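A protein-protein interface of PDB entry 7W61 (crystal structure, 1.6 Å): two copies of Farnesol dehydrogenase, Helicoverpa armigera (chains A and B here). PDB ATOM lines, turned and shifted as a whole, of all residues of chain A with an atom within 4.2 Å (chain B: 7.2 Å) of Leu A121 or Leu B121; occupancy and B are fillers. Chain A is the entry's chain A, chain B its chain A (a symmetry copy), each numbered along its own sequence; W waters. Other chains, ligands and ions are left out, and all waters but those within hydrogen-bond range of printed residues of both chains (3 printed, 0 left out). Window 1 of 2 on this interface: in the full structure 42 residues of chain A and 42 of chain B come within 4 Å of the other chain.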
ATOM      1  N   VAL A 116     -14.115  28.946  12.180  1.00  0.00           N
ATOM      2  CA  VAL A 116     -13.580  27.573  12.096  1.00  0.00           C
ATOM      3  C   VAL A 116     -12.291  27.486  12.933  1.00  0.00           C
ATOM      4  O   VAL A 116     -12.040  26.519  13.720  1.00  0.00           O
ATOM      5  CB  VAL A 116     -13.302  27.151  10.641  1.00  0.00           C
ATOM      6  CG1 VAL A 116     -12.730  25.699  10.642  1.00  0.00           C
ATOM      7  CG2 VAL A 116     -14.498  27.101   9.694  1.00  0.00           C
ATOM      8  N   ILE A 117     -11.419  28.538  12.859  1.00  0.00           N
ATOM      9  CA  ILE A 117     -10.230  28.492  13.706  1.00  0.00           C
ATOM     10  C   ILE A 117     -10.615  28.582  15.202  1.00  0.00           C
ATOM     11  O   ILE A 117     -10.016  27.900  16.049  1.00  0.00           O
ATOM     12  CB  ILE A 117      -9.301  29.676  13.316  1.00  0.00           C
ATOM     13  CG1 ILE A 117      -8.920  29.607  11.817  1.00  0.00           C
ATOM     14  CG2 ILE A 117      -8.045  29.597  14.191  1.00  0.00           C
ATOM     15  CD1 ILE A 117      -8.266  28.295  11.347  1.00  0.00           C
ATOM     16  N   ILE A 119     -13.407  27.826  16.896  1.00  0.00           N
ATOM     17  CA  ILE A 119     -14.034  26.640  17.491  1.00  0.00           C
ATOM     18  C   ILE A 119     -13.059  25.447  17.445  1.00  0.00           C
ATOM     19  O   ILE A 119     -12.910  24.740  18.424  1.00  0.00           O
ATOM     20  CB  ILE A 119     -15.342  26.301  16.712  1.00  0.00           C
ATOM     21  CG1 ILE A 119     -16.270  27.500  16.931  1.00  0.00           C
ATOM     22  CG2 ILE A 119     -15.973  24.998  17.253  1.00  0.00           C
ATOM     23  CD1 ILE A 119     -17.545  27.443  16.083  1.00  0.00           C
ATOM     24  N   ASN A 120     -12.493  25.175  16.276  1.00  0.00           N
ATOM     25  CA  ASN A 120     -11.814  23.881  16.136  1.00  0.00           C
ATOM     26  C   ASN A 120     -10.420  23.907  16.760  1.00  0.00           C
ATOM     27  O   ASN A 120      -9.886  22.815  17.062  1.00  0.00           O
ATOM     28  CB  ASN A 120     -11.562  23.575  14.617  1.00  0.00           C
ATOM     29  CG  ASN A 120     -12.856  23.228  13.899  1.00  0.00           C
ATOM     30  OD1 ASN A 120     -13.959  23.379  14.447  1.00  0.00           O
ATOM     31  ND2 ASN A 120     -12.773  22.805  12.649  1.00  0.00           N
ATOM     32  N   LEU A 121      -9.783  25.090  16.902  1.00  0.00           N
ATOM     33  CA  LEU A 121      -8.440  25.116  17.479  1.00  0.00           C
ATOM     34  C   LEU A 121      -8.422  25.876  18.798  1.00  0.00           C
ATOM     35  O   LEU A 121      -7.874  25.329  19.767  1.00  0.00           O
ATOM     36  CB  LEU A 121      -7.480  25.696  16.419  1.00  0.00           C
ATOM     37  CG  LEU A 121      -6.011  25.857  16.903  1.00  0.00           C
ATOM     38  CD1 LEU A 121      -5.461  24.501  17.369  1.00  0.00           C
ATOM     39  CD2 LEU A 121      -5.147  26.407  15.738  1.00  0.00           C
ATOM     40  N   LYS A 122      -8.996  27.100  18.838  1.00  0.00           N
ATOM     41  CA  LYS A 122      -8.973  27.804  20.127  1.00  0.00           C
ATOM     42  C   LYS A 122      -9.775  27.032  21.163  1.00  0.00           C
ATOM     43  O   LYS A 122      -9.375  27.030  22.337  1.00  0.00           O
ATOM     44  CB  LYS A 122      -9.257  29.322  20.006  1.00  0.00           C
ATOM     45  CG  LYS A 122      -8.117  30.026  19.260  1.00  0.00           C
ATOM     46  CD  LYS A 122      -8.421  31.322  18.436  1.00  0.00           C
ATOM     47  CE  LYS A 122      -8.785  32.337  19.476  1.00  0.00           C
ATOM     48  NZ  LYS A 122      -9.136  33.720  18.982  1.00  0.00           N
ATOM     49  N   GLY A 123     -10.903  26.420  20.783  1.00  0.00           N
ATOM     50  CA  GLY A 123     -11.812  25.773  21.718  1.00  0.00           C
ATOM     51  C   GLY A 123     -11.047  24.706  22.485  1.00  0.00           C
ATOM     52  O   GLY A 123     -11.097  24.664  23.736  1.00  0.00           O
ATOM     53  N   PRO A 124     -10.376  23.767  21.820  1.00  0.00           N
ATOM     54  CA  PRO A 124      -9.654  22.752  22.570  1.00  0.00           C
ATOM     55  C   PRO A 124      -8.508  23.288  23.438  1.00  0.00           C
ATOM     56  O   PRO A 124      -8.215  22.722  24.492  1.00  0.00           O
ATOM     57  CB  PRO A 124      -9.066  21.879  21.434  1.00  0.00           C
ATOM     58  CG  PRO A 124     -10.224  21.996  20.408  1.00  0.00           C
ATOM     59  CD  PRO A 124     -10.490  23.479  20.358  1.00  0.00           C
ATOM     60  N   ILE A 125      -7.851  24.387  23.008  1.00  0.00           N
ATOM     61  CA  ILE A 125      -6.814  25.017  23.850  1.00  0.00           C
ATOM     62  C   ILE A 125      -7.426  25.534  25.145  1.00  0.00           C
ATOM     63  O   ILE A 125      -6.905  25.235  26.224  1.00  0.00           O
ATOM     64  CB  ILE A 125      -6.101  26.161  23.084  1.00  0.00           C
ATOM     65  CG1 ILE A 125      -5.366  25.541  21.901  1.00  0.00           C
ATOM     66  CG2 ILE A 125      -5.142  26.939  24.032  1.00  0.00           C
ATOM     67  CD1 ILE A 125      -4.875  26.596  20.861  1.00  0.00           C
ATOM     68  N   SER A 166      -6.287  23.404   7.922  1.00  0.00           N
ATOM     69  CA  SER A 166      -5.396  24.222   8.751  1.00  0.00           C
ATOM     70  C   SER A 166      -5.783  24.100  10.230  1.00  0.00           C
ATOM     71  O   SER A 166      -4.886  23.920  11.081  1.00  0.00           O
ATOM     72  CB  SER A 166      -5.567  25.655   8.304  1.00  0.00           C
ATOM     73  OG  SER A 166      -4.784  26.565   9.112  1.00  0.00           O
ATOM     74  N   SER A 167      -7.077  24.154  10.563  1.00  0.00           N
ATOM     75  CA  SER A 167      -7.429  24.107  11.975  1.00  0.00           C
ATOM     76  C   SER A 167      -7.028  22.755  12.571  1.00  0.00           C
ATOM     77  O   SER A 167      -6.657  22.716  13.723  1.00  0.00           O
ATOM     78  CB  SER A 167      -8.948  24.404  12.129  1.00  0.00           C
ATOM     79  OG  SER A 167      -9.768  23.274  11.781  1.00  0.00           O
ATOM     80  N   GLY A 170      -3.415  22.442  13.050  1.00  0.00           N
ATOM     81  CA  GLY A 170      -3.256  23.160  14.320  1.00  0.00           C
ATOM     82  C   GLY A 170      -3.475  22.198  15.493  1.00  0.00           C
ATOM     83  O   GLY A 170      -2.752  22.159  16.512  1.00  0.00           O
ATOM     84  N   LEU A 171      -4.591  21.459  15.423  1.00  0.00           N
ATOM     85  CA  LEU A 171      -4.909  20.569  16.558  1.00  0.00           C
ATOM     86  C   LEU A 171      -3.918  19.419  16.677  1.00  0.00           C
ATOM     87  O   LEU A 171      -3.577  19.007  17.771  1.00  0.00           O
ATOM     88  CB  LEU A 171      -6.343  20.052  16.309  1.00  0.00           C
ATOM     89  CG  LEU A 171      -6.893  19.284  17.522  1.00  0.00           C
ATOM     90  CD1 LEU A 171      -7.163  20.222  18.674  1.00  0.00           C
ATOM     91  CD2 LEU A 171      -8.248  18.595  17.151  1.00  0.00           C
ATOM     92  N   ALA B  92       4.505  38.823   9.918  1.00  0.00           N
ATOM     93  CA  ALA B  92       4.326  39.148  11.338  1.00  0.00           C
ATOM     94  C   ALA B  92       4.087  37.841  12.122  1.00  0.00           C
ATOM     95  O   ALA B  92       3.339  36.956  11.687  1.00  0.00           O
ATOM     96  CB  ALA B  92       3.114  40.058  11.508  1.00  0.00           C
ATOM     97  N   MET B 114      -4.057  33.079  23.311  1.00  0.00           N
ATOM     98  CA  MET B 114      -4.960  33.397  22.199  1.00  0.00           C
ATOM     99  C   MET B 114      -4.311  34.270  21.132  1.00  0.00           C
ATOM    100  O   MET B 114      -4.521  34.023  19.937  1.00  0.00           O
ATOM    101  CB  MET B 114      -6.216  34.068  22.737  1.00  0.00           C
ATOM    102  CG  MET B 114      -7.065  33.102  23.631  1.00  0.00           C
ATOM    103  SD  MET B 114      -7.826  31.624  22.814  1.00  0.00           S
ATOM    104  CE  MET B 114      -6.671  30.310  23.144  1.00  0.00           C
ATOM    105  N   SER B 115      -3.478  35.217  21.553  1.00  0.00           N
ATOM    106  CA  SER B 115      -2.787  36.118  20.636  1.00  0.00           C
ATOM    107  C   SER B 115      -1.893  35.357  19.670  1.00  0.00           C
ATOM    108  O   SER B 115      -1.832  35.713  18.461  1.00  0.00           O
ATOM    109  CB  SER B 115      -1.927  37.141  21.388  1.00  0.00           C
ATOM    110  OG  SER B 115      -2.773  38.101  21.964  1.00  0.00           O
ATOM    111  N   VAL B 116      -1.222  34.302  20.176  1.00  0.00           N
ATOM    112  CA  VAL B 116      -0.285  33.607  19.273  1.00  0.00           C
ATOM    113  C   VAL B 116      -1.078  32.996  18.103  1.00  0.00           C
ATOM    114  O   VAL B 116      -0.698  33.076  16.892  1.00  0.00           O
ATOM    115  CB  VAL B 116       0.515  32.513  20.003  1.00  0.00           C
ATOM    116  CG1 VAL B 116       1.469  31.821  18.979  1.00  0.00           C
ATOM    117  CG2 VAL B 116       1.425  32.965  21.143  1.00  0.00           C
ATOM    118  N   ILE B 117      -2.276  32.401  18.394  1.00  0.00           N
ATOM    119  CA  ILE B 117      -3.064  31.885  17.279  1.00  0.00           C
ATOM    120  C   ILE B 117      -3.564  33.038  16.376  1.00  0.00           C
ATOM    121  O   ILE B 117      -3.586  32.909  15.142  1.00  0.00           O
ATOM    122  CB  ILE B 117      -4.270  31.089  17.855  1.00  0.00           C
ATOM    123  CG1 ILE B 117      -3.784  29.941  18.772  1.00  0.00           C
ATOM    124  CG2 ILE B 117      -5.070  30.528  16.674  1.00  0.00           C
ATOM    125  CD1 ILE B 117      -2.795  28.944  18.140  1.00  0.00           C
ATOM    126  N   ASP B 118      -4.090  34.105  17.004  1.00  0.00           N
ATOM    127  CA  ASP B 118      -4.712  35.183  16.218  1.00  0.00           C
ATOM    128  C   ASP B 118      -3.663  35.809  15.291  1.00  0.00           C
ATOM    129  O   ASP B 118      -3.998  36.160  14.155  1.00  0.00           O
ATOM    130  CB  ASP B 118      -5.274  36.215  17.197  1.00  0.00           C
ATOM    131  CG  ASP B 118      -6.541  35.723  17.850  1.00  0.00           C
ATOM    132  OD1 ASP B 118      -7.089  34.653  17.439  1.00  0.00           O
ATOM    133  OD2 ASP B 118      -6.884  36.393  18.835  1.00  0.00           O
ATOM    134  N   ILE B 119      -2.446  36.146  15.806  1.00  0.00           N
ATOM    135  CA  ILE B 119      -1.445  36.807  14.960  1.00  0.00           C
ATOM    136  C   ILE B 119      -0.854  35.799  13.956  1.00  0.00           C
ATOM    137  O   ILE B 119      -0.718  36.107  12.786  1.00  0.00           O
ATOM    138  CB  ILE B 119      -0.317  37.400  15.860  1.00  0.00           C
ATOM    139  CG1 ILE B 119      -1.001  38.465  16.722  1.00  0.00           C
ATOM    140  CG2 ILE B 119       0.803  38.015  14.991  1.00  0.00           C
ATOM    141  CD1 ILE B 119      -0.091  39.035  17.816  1.00  0.00           C
ATOM    142  N   ASN B 120      -0.407  34.649  14.445  1.00  0.00           N
ATOM    143  CA  ASN B 120       0.427  33.817  13.570  1.00  0.00           C
ATOM    144  C   ASN B 120      -0.419  33.020  12.578  1.00  0.00           C
ATOM    145  O   ASN B 120       0.136  32.581  11.545  1.00  0.00           O
ATOM    146  CB  ASN B 120       1.168  32.727  14.422  1.00  0.00           C
ATOM    147  CG  ASN B 120       2.273  33.340  15.267  1.00  0.00           C
ATOM    148  OD1 ASN B 120       2.393  34.569  15.379  1.00  0.00           O
ATOM    149  ND2 ASN B 120       3.074  32.518  15.923  1.00  0.00           N
ATOM    150  N   LEU B 121      -1.710  32.757  12.875  1.00  0.00           N
ATOM    151  CA  LEU B 121      -2.517  31.977  11.938  1.00  0.00           C
ATOM    152  C   LEU B 121      -3.664  32.804  11.377  1.00  0.00           C
ATOM    153  O   LEU B 121      -3.823  32.805  10.147  1.00  0.00           O
ATOM    154  CB  LEU B 121      -2.977  30.694  12.663  1.00  0.00           C
ATOM    155  CG  LEU B 121      -3.910  29.780  11.819  1.00  0.00           C
ATOM    156  CD1 LEU B 121      -3.209  29.377  10.513  1.00  0.00           C
ATOM    157  CD2 LEU B 121      -4.264  28.513  12.642  1.00  0.00           C
ATOM    158  N   LYS B 122      -4.446  33.485  12.246  1.00  0.00           N
ATOM    159  CA  LYS B 122      -5.538  34.284  11.675  1.00  0.00           C
ATOM    160  C   LYS B 122      -4.978  35.394  10.801  1.00  0.00           C
ATOM    161  O   LYS B 122      -5.602  35.712   9.778  1.00  0.00           O
ATOM    162  CB  LYS B 122      -6.618  34.683  12.711  1.00  0.00           C
ATOM    163  CG  LYS B 122      -7.378  33.444  13.202  1.00  0.00           C
ATOM    164  CD  LYS B 122      -7.993  33.438  14.642  1.00  0.00           C
ATOM    165  CE  LYS B 122      -9.081  34.465  14.577  1.00  0.00           C
ATOM    166  NZ  LYS B 122      -9.876  34.693  15.841  1.00  0.00           N
ATOM    167  N   GLY B 123      -3.857  36.017  11.186  1.00  0.00           N
ATOM    168  CA  GLY B 123      -3.314  37.178  10.496  1.00  0.00           C
ATOM    169  C   GLY B 123      -3.058  36.809   9.044  1.00  0.00           C
ATOM    170  O   GLY B 123      -3.493  37.533   8.118  1.00  0.00           O
ATOM    171  N   PRO B 124      -2.305  35.749   8.754  1.00  0.00           N
ATOM    172  CA  PRO B 124      -2.067  35.414   7.360  1.00  0.00           C
ATOM    173  C   PRO B 124      -3.323  35.034   6.566  1.00  0.00           C
ATOM    174  O   PRO B 124      -3.394  35.287   5.362  1.00  0.00           O
ATOM    175  CB  PRO B 124      -1.150  34.172   7.486  1.00  0.00           C
ATOM    176  CG  PRO B 124      -0.363  34.576   8.760  1.00  0.00           C
ATOM    177  CD  PRO B 124      -1.449  34.993   9.718  1.00  0.00           C
ATOM    178  N   ILE B 125      -4.331  34.426   7.230  1.00  0.00           N
ATOM    179  CA  ILE B 125      -5.609  34.135   6.551  1.00  0.00           C
ATOM    180  C   ILE B 125      -6.285  35.430   6.121  1.00  0.00           C
ATOM    181  O   ILE B 125      -6.680  35.550   4.956  1.00  0.00           O
ATOM    182  CB  ILE B 125      -6.544  33.304   7.466  1.00  0.00           C
ATOM    183  CG1 ILE B 125      -5.878  31.954   7.708  1.00  0.00           C
ATOM    184  CG2 ILE B 125      -7.953  33.158   6.819  1.00  0.00           C
ATOM    185  CD1 ILE B 125      -6.540  31.141   8.863  1.00  0.00           C
ATOM    186  N   LEU B 126      -6.381  36.400   7.051  1.00  0.00           N
ATOM    187  CA  LEU B 126      -7.086  37.644   6.706  1.00  0.00           C
ATOM    188  C   LEU B 126      -6.296  38.406   5.607  1.00  0.00           C
ATOM    189  O   LEU B 126      -6.885  38.917   4.652  1.00  0.00           O
ATOM    190  CB  LEU B 126      -7.178  38.552   7.963  1.00  0.00           C
ATOM    191  CG  LEU B 126      -8.108  37.998   9.058  1.00  0.00           C
ATOM    192  CD1 LEU B 126      -7.902  38.771  10.376  1.00  0.00           C
ATOM    193  CD2 LEU B 126      -9.576  38.070   8.611  1.00  0.00           C
ATOM    194  N   VAL B 163       1.707  26.841  22.219  1.00  0.00           N
ATOM    195  CA  VAL B 163       0.942  26.647  20.992  1.00  0.00           C
ATOM    196  C   VAL B 163       1.615  27.309  19.796  1.00  0.00           C
ATOM    197  O   VAL B 163       0.994  27.445  18.738  1.00  0.00           O
ATOM    198  CB  VAL B 163      -0.486  27.210  21.127  1.00  0.00           C
ATOM    199  CG1 VAL B 163      -1.188  26.609  22.345  1.00  0.00           C
ATOM    200  CG2 VAL B 163      -0.523  28.731  21.292  1.00  0.00           C
ATOM    201  N   SER B 166       1.737  24.685  17.196  1.00  0.00           N
ATOM    202  CA  SER B 166       0.370  24.536  16.686  1.00  0.00           C
ATOM    203  C   SER B 166       0.052  25.649  15.681  1.00  0.00           C
ATOM    204  O   SER B 166      -0.507  25.354  14.603  1.00  0.00           O
ATOM    205  CB  SER B 166      -0.560  24.649  17.872  1.00  0.00           C
ATOM    206  OG  SER B 166      -1.949  24.591  17.470  1.00  0.00           O
ATOM    207  N   SER B 167       0.415  26.902  15.971  1.00  0.00           N
ATOM    208  CA  SER B 167       0.047  27.962  15.043  1.00  0.00           C
ATOM    209  C   SER B 167       0.756  27.754  13.703  1.00  0.00           C
ATOM    210  O   SER B 167       0.182  28.077  12.687  1.00  0.00           O
ATOM    211  CB  SER B 167       0.375  29.339  15.689  1.00  0.00           C
ATOM    212  OG  SER B 167       1.779  29.647  15.644  1.00  0.00           O
ATOM    213  N   LYS B 168       2.024  27.281  13.742  1.00  0.00           N
ATOM    214  CA  LYS B 168       2.795  27.125  12.495  1.00  0.00           C
ATOM    215  C   LYS B 168       2.385  25.856  11.739  1.00  0.00           C
ATOM    216  O   LYS B 168       2.412  25.888  10.494  1.00  0.00           O
ATOM    217  CB  LYS B 168       4.309  27.182  12.792  1.00  0.00           C
ATOM    218  CG  LYS B 168       4.723  28.574  13.361  1.00  0.00           C
ATOM    219  CD  LYS B 168       4.683  29.710  12.312  1.00  0.00           C
ATOM    220  CE  LYS B 168       5.484  30.901  12.782  1.00  0.00           C
ATOM    221  NZ  LYS B 168       5.398  32.061  11.824  1.00  0.00           N
ATOM    222  N   TYR B 169       1.989  24.778  12.453  1.00  0.00           N
ATOM    223  CA  TYR B 169       1.337  23.648  11.778  1.00  0.00           C
ATOM    224  C   TYR B 169       0.075  24.128  11.063  1.00  0.00           C
ATOM    225  O   TYR B 169      -0.160  23.761   9.896  1.00  0.00           O
ATOM    226  CB  TYR B 169       0.895  22.575  12.797  1.00  0.00           C
ATOM    227  CG  TYR B 169       1.942  21.506  13.063  1.00  0.00           C
ATOM    228  CD1 TYR B 169       3.204  21.807  13.555  1.00  0.00           C
ATOM    229  CD2 TYR B 169       1.667  20.173  12.736  1.00  0.00           C
ATOM    230  CE1 TYR B 169       4.153  20.827  13.790  1.00  0.00           C
ATOM    231  CE2 TYR B 169       2.612  19.157  12.940  1.00  0.00           C
ATOM    232  CZ  TYR B 169       3.851  19.520  13.504  1.00  0.00           C
ATOM    233  OH  TYR B 169       4.848  18.543  13.676  1.00  0.00           O
ATOM    234  N   GLY B 170      -0.678  25.005  11.761  1.00  0.00           N
ATOM    235  CA  GLY B 170      -1.831  25.684  11.158  1.00  0.00           C
ATOM    236  C   GLY B 170      -1.410  26.362   9.850  1.00  0.00           C
ATOM    237  O   GLY B 170      -2.079  26.324   8.794  1.00  0.00           O
ATOM    238  N   LEU B 171      -0.312  27.126   9.932  1.00  0.00           N
ATOM    239  CA  LEU B 171       0.106  27.875   8.729  1.00  0.00           C
ATOM    240  C   LEU B 171       0.591  26.952   7.621  1.00  0.00           C
ATOM    241  O   LEU B 171       0.358  27.211   6.453  1.00  0.00           O
ATOM    242  CB  LEU B 171       1.224  28.836   9.190  1.00  0.00           C
ATOM    243  CG  LEU B 171       1.608  29.838   8.089  1.00  0.00           C
ATOM    244  CD1 LEU B 171       0.499  30.837   7.862  1.00  0.00           C
ATOM    245  CD2 LEU B 171       2.882  30.640   8.514  1.00  0.00           C
ATOM    246  N   THR B 172       1.215  25.811   7.954  1.00  0.00           N
ATOM    247  CA  THR B 172       1.599  24.832   6.913  1.00  0.00           C
ATOM    248  C   THR B 172       0.345  24.339   6.158  1.00  0.00           C
ATOM    249  O   THR B 172       0.303  24.316   4.922  1.00  0.00           O
ATOM    250  CB  THR B 172       2.293  23.634   7.573  1.00  0.00           C
ATOM    251  OG1 THR B 172       3.529  24.093   8.103  1.00  0.00           O
ATOM    252  CG2 THR B 172       2.603  22.552   6.552  1.00  0.00           C
ATOM    253  N   GLY B 173      -0.671  23.960   6.949  1.00  0.00           N
ATOM    254  CA  GLY B 173      -1.883  23.477   6.316  1.00  0.00           C
ATOM    255  C   GLY B 173      -2.624  24.562   5.541  1.00  0.00           C
ATOM    256  O   GLY B 173      -3.119  24.259   4.430  1.00  0.00           O
ATOM    257  N   PHE B 174      -2.683  25.773   6.143  1.00  0.00           N
ATOM    258  CA  PHE B 174      -3.294  26.902   5.427  1.00  0.00           C
ATOM    259  C   PHE B 174      -2.632  27.138   4.082  1.00  0.00           C
ATOM    260  O   PHE B 174      -3.279  27.314   3.043  1.00  0.00           O
ATOM    261  CB  PHE B 174      -3.250  28.179   6.293  1.00  0.00           C
ATOM    262  CG  PHE B 174      -3.639  29.407   5.478  1.00  0.00           C
ATOM    263  CD1 PHE B 174      -4.950  29.513   4.998  1.00  0.00           C
ATOM    264  CD2 PHE B 174      -2.728  30.443   5.279  1.00  0.00           C
ATOM    265  CE1 PHE B 174      -5.343  30.644   4.249  1.00  0.00           C
ATOM    266  CE2 PHE B 174      -3.132  31.560   4.562  1.00  0.00           C
ATOM    267  CZ  PHE B 174      -4.372  31.570   4.007  1.00  0.00           C
ATOM    268  N   SER B 175      -1.302  27.243   4.113  1.00  0.00           N
ATOM    269  CA  SER B 175      -0.552  27.578   2.902  1.00  0.00           C
ATOM    270  C   SER B 175      -0.853  26.567   1.806  1.00  0.00           C
ATOM    271  O   SER B 175      -1.053  26.904   0.607  1.00  0.00           O
ATOM    272  CB  SER B 175       0.968  27.558   3.194  1.00  0.00           C
ATOM    273  OG  SER B 175       1.266  28.617   4.065  1.00  0.00           O
HETATM  274  O   HOH W   1     -11.401  34.785  18.686  1.00  0.00           O
HETATM  275  O   HOH W   2      -9.759  34.463  21.967  1.00  0.00           O
HETATM  276  O   HOH W   3      -9.692  36.552  17.533  1.00  0.00           O
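CG2 of Ile A117 touches CG2 of Ile B117 (3.99 Å). Ile A117 touches Lys B122 (CG2 to CD, 3.9 Å). Leu A121 touches Leu B121. Ser B166 touches Leu A121 (OG to CD1, 3.5 Å). Lys A122 touches Met B114 (CE to SD, 3.5 Å). Ile B117 touches Lys A122. CE of Met B114 touches CG2 of Ile A125, at 3.8 Å. CG1 of Val B163 touches CD1 of Ile A125, 3.97 Å away. Leu B121 touches Ser A166 (CD1 to OG, 3.5 Å). N of Gly B170 touches N of Gly A170, at 3.97 Å.
Of chain B, only Leu B121 and Ser B166 come within 4 Å of Leu A121. Leu B121 touches two residues of chain A. Printed residues of chain A within 4 Å of Phe B174: Ser A166. Of the printed residues of chain B, Ser A166 touches Leu B121 (3.5 Å), Gly B170 (2.7 Å) and Phe B174 (3.6 Å). Leu B126 touches none of the printed residues of chain A. The nearest residue of chain B that does not touch Leu A121 is Ile B117 (4.2 Å). The nearest printed residue of chain A that does not touch Ile B117 is Ile A125 (4.1 Å).
Ile B117 touches its own counterpart, Ile A117. Ile A117 touches Lys B122, and with the chains exchanged Lys A122 touches Ile B117. Leu A121 touches its own counterpart, Leu B121. Gly B170 touches its own counterpart, Gly A170. 13 positions are printed for both chains.
Water W1 lies within hydrogen-bond range of the side-chain amino group (NZ) of Lys A122 (2.5 Å) and the side-chain amino group (NZ) of Lys B122 (3.2 Å). Water W3 lies within hydrogen-bond range of NZ of Lys B122, OD2 of Asp B118 and NZ of Lys A122. Water W2 bridges the side-chain amino group of Lys A122 and the side-chain sulfur of Met B114.
NZ of Lys A122 lies within salt-bridge range of OD1 of Asp B118. OG of Ser A166 lies within hydrogen-bond range of O of Gly B170 (2.7 Å). The backbone carbonyl oxygen (O) of Gly A170 sits at hydrogen-bond distance from the side-chain hydroxyl (OG) of Ser B166. The side-chain amino group (NZ) of Lys B122 lies close to the side-chain amino group (NZ) of Lys A122 (3.4 Å).
The backbone NH of Gly B123 lies within hydrogen-bond range of the backbone carbonyl oxygen of Asp B118 (3.0 Å). The backbone carbonyl oxygen of Ile A117 is in hydrogen-bond range of the backbone NH of Lys A122 (3.1 Å). The side-chain carboxylate (OD1) of Asp B118 lies within salt-bridge range of the side-chain amino group (NZ) of Lys B122 (3.2 Å). O of Ile B117 is in hydrogen-bond range of N of Lys B122 (3.1 Å).
Printed residues of chain A that touch a printed residue of chain B: Ile A117, Leu A121, Lys A122, Ile A125, Ser A166 and Gly A170. Along chain A the printed residues that touch a printed residue of chain B span positions 117 to 170. Of the 25 printed residues of chain B, 9 touch a printed residue of chain A. Hydrophobic or aromatic side chains of chain B that line the printed part of chain A: Met B114, Ile B117, Leu B121, Val B163 and Phe B174. Among the printed residues, 15 pairs touch across the chains. Among the printed residues, Asp or Glu carboxylates within 4 Å of a Lys or Arg side-chain nitrogen of the other chain: Lys A122 with Asp B118 (2.7 Å).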
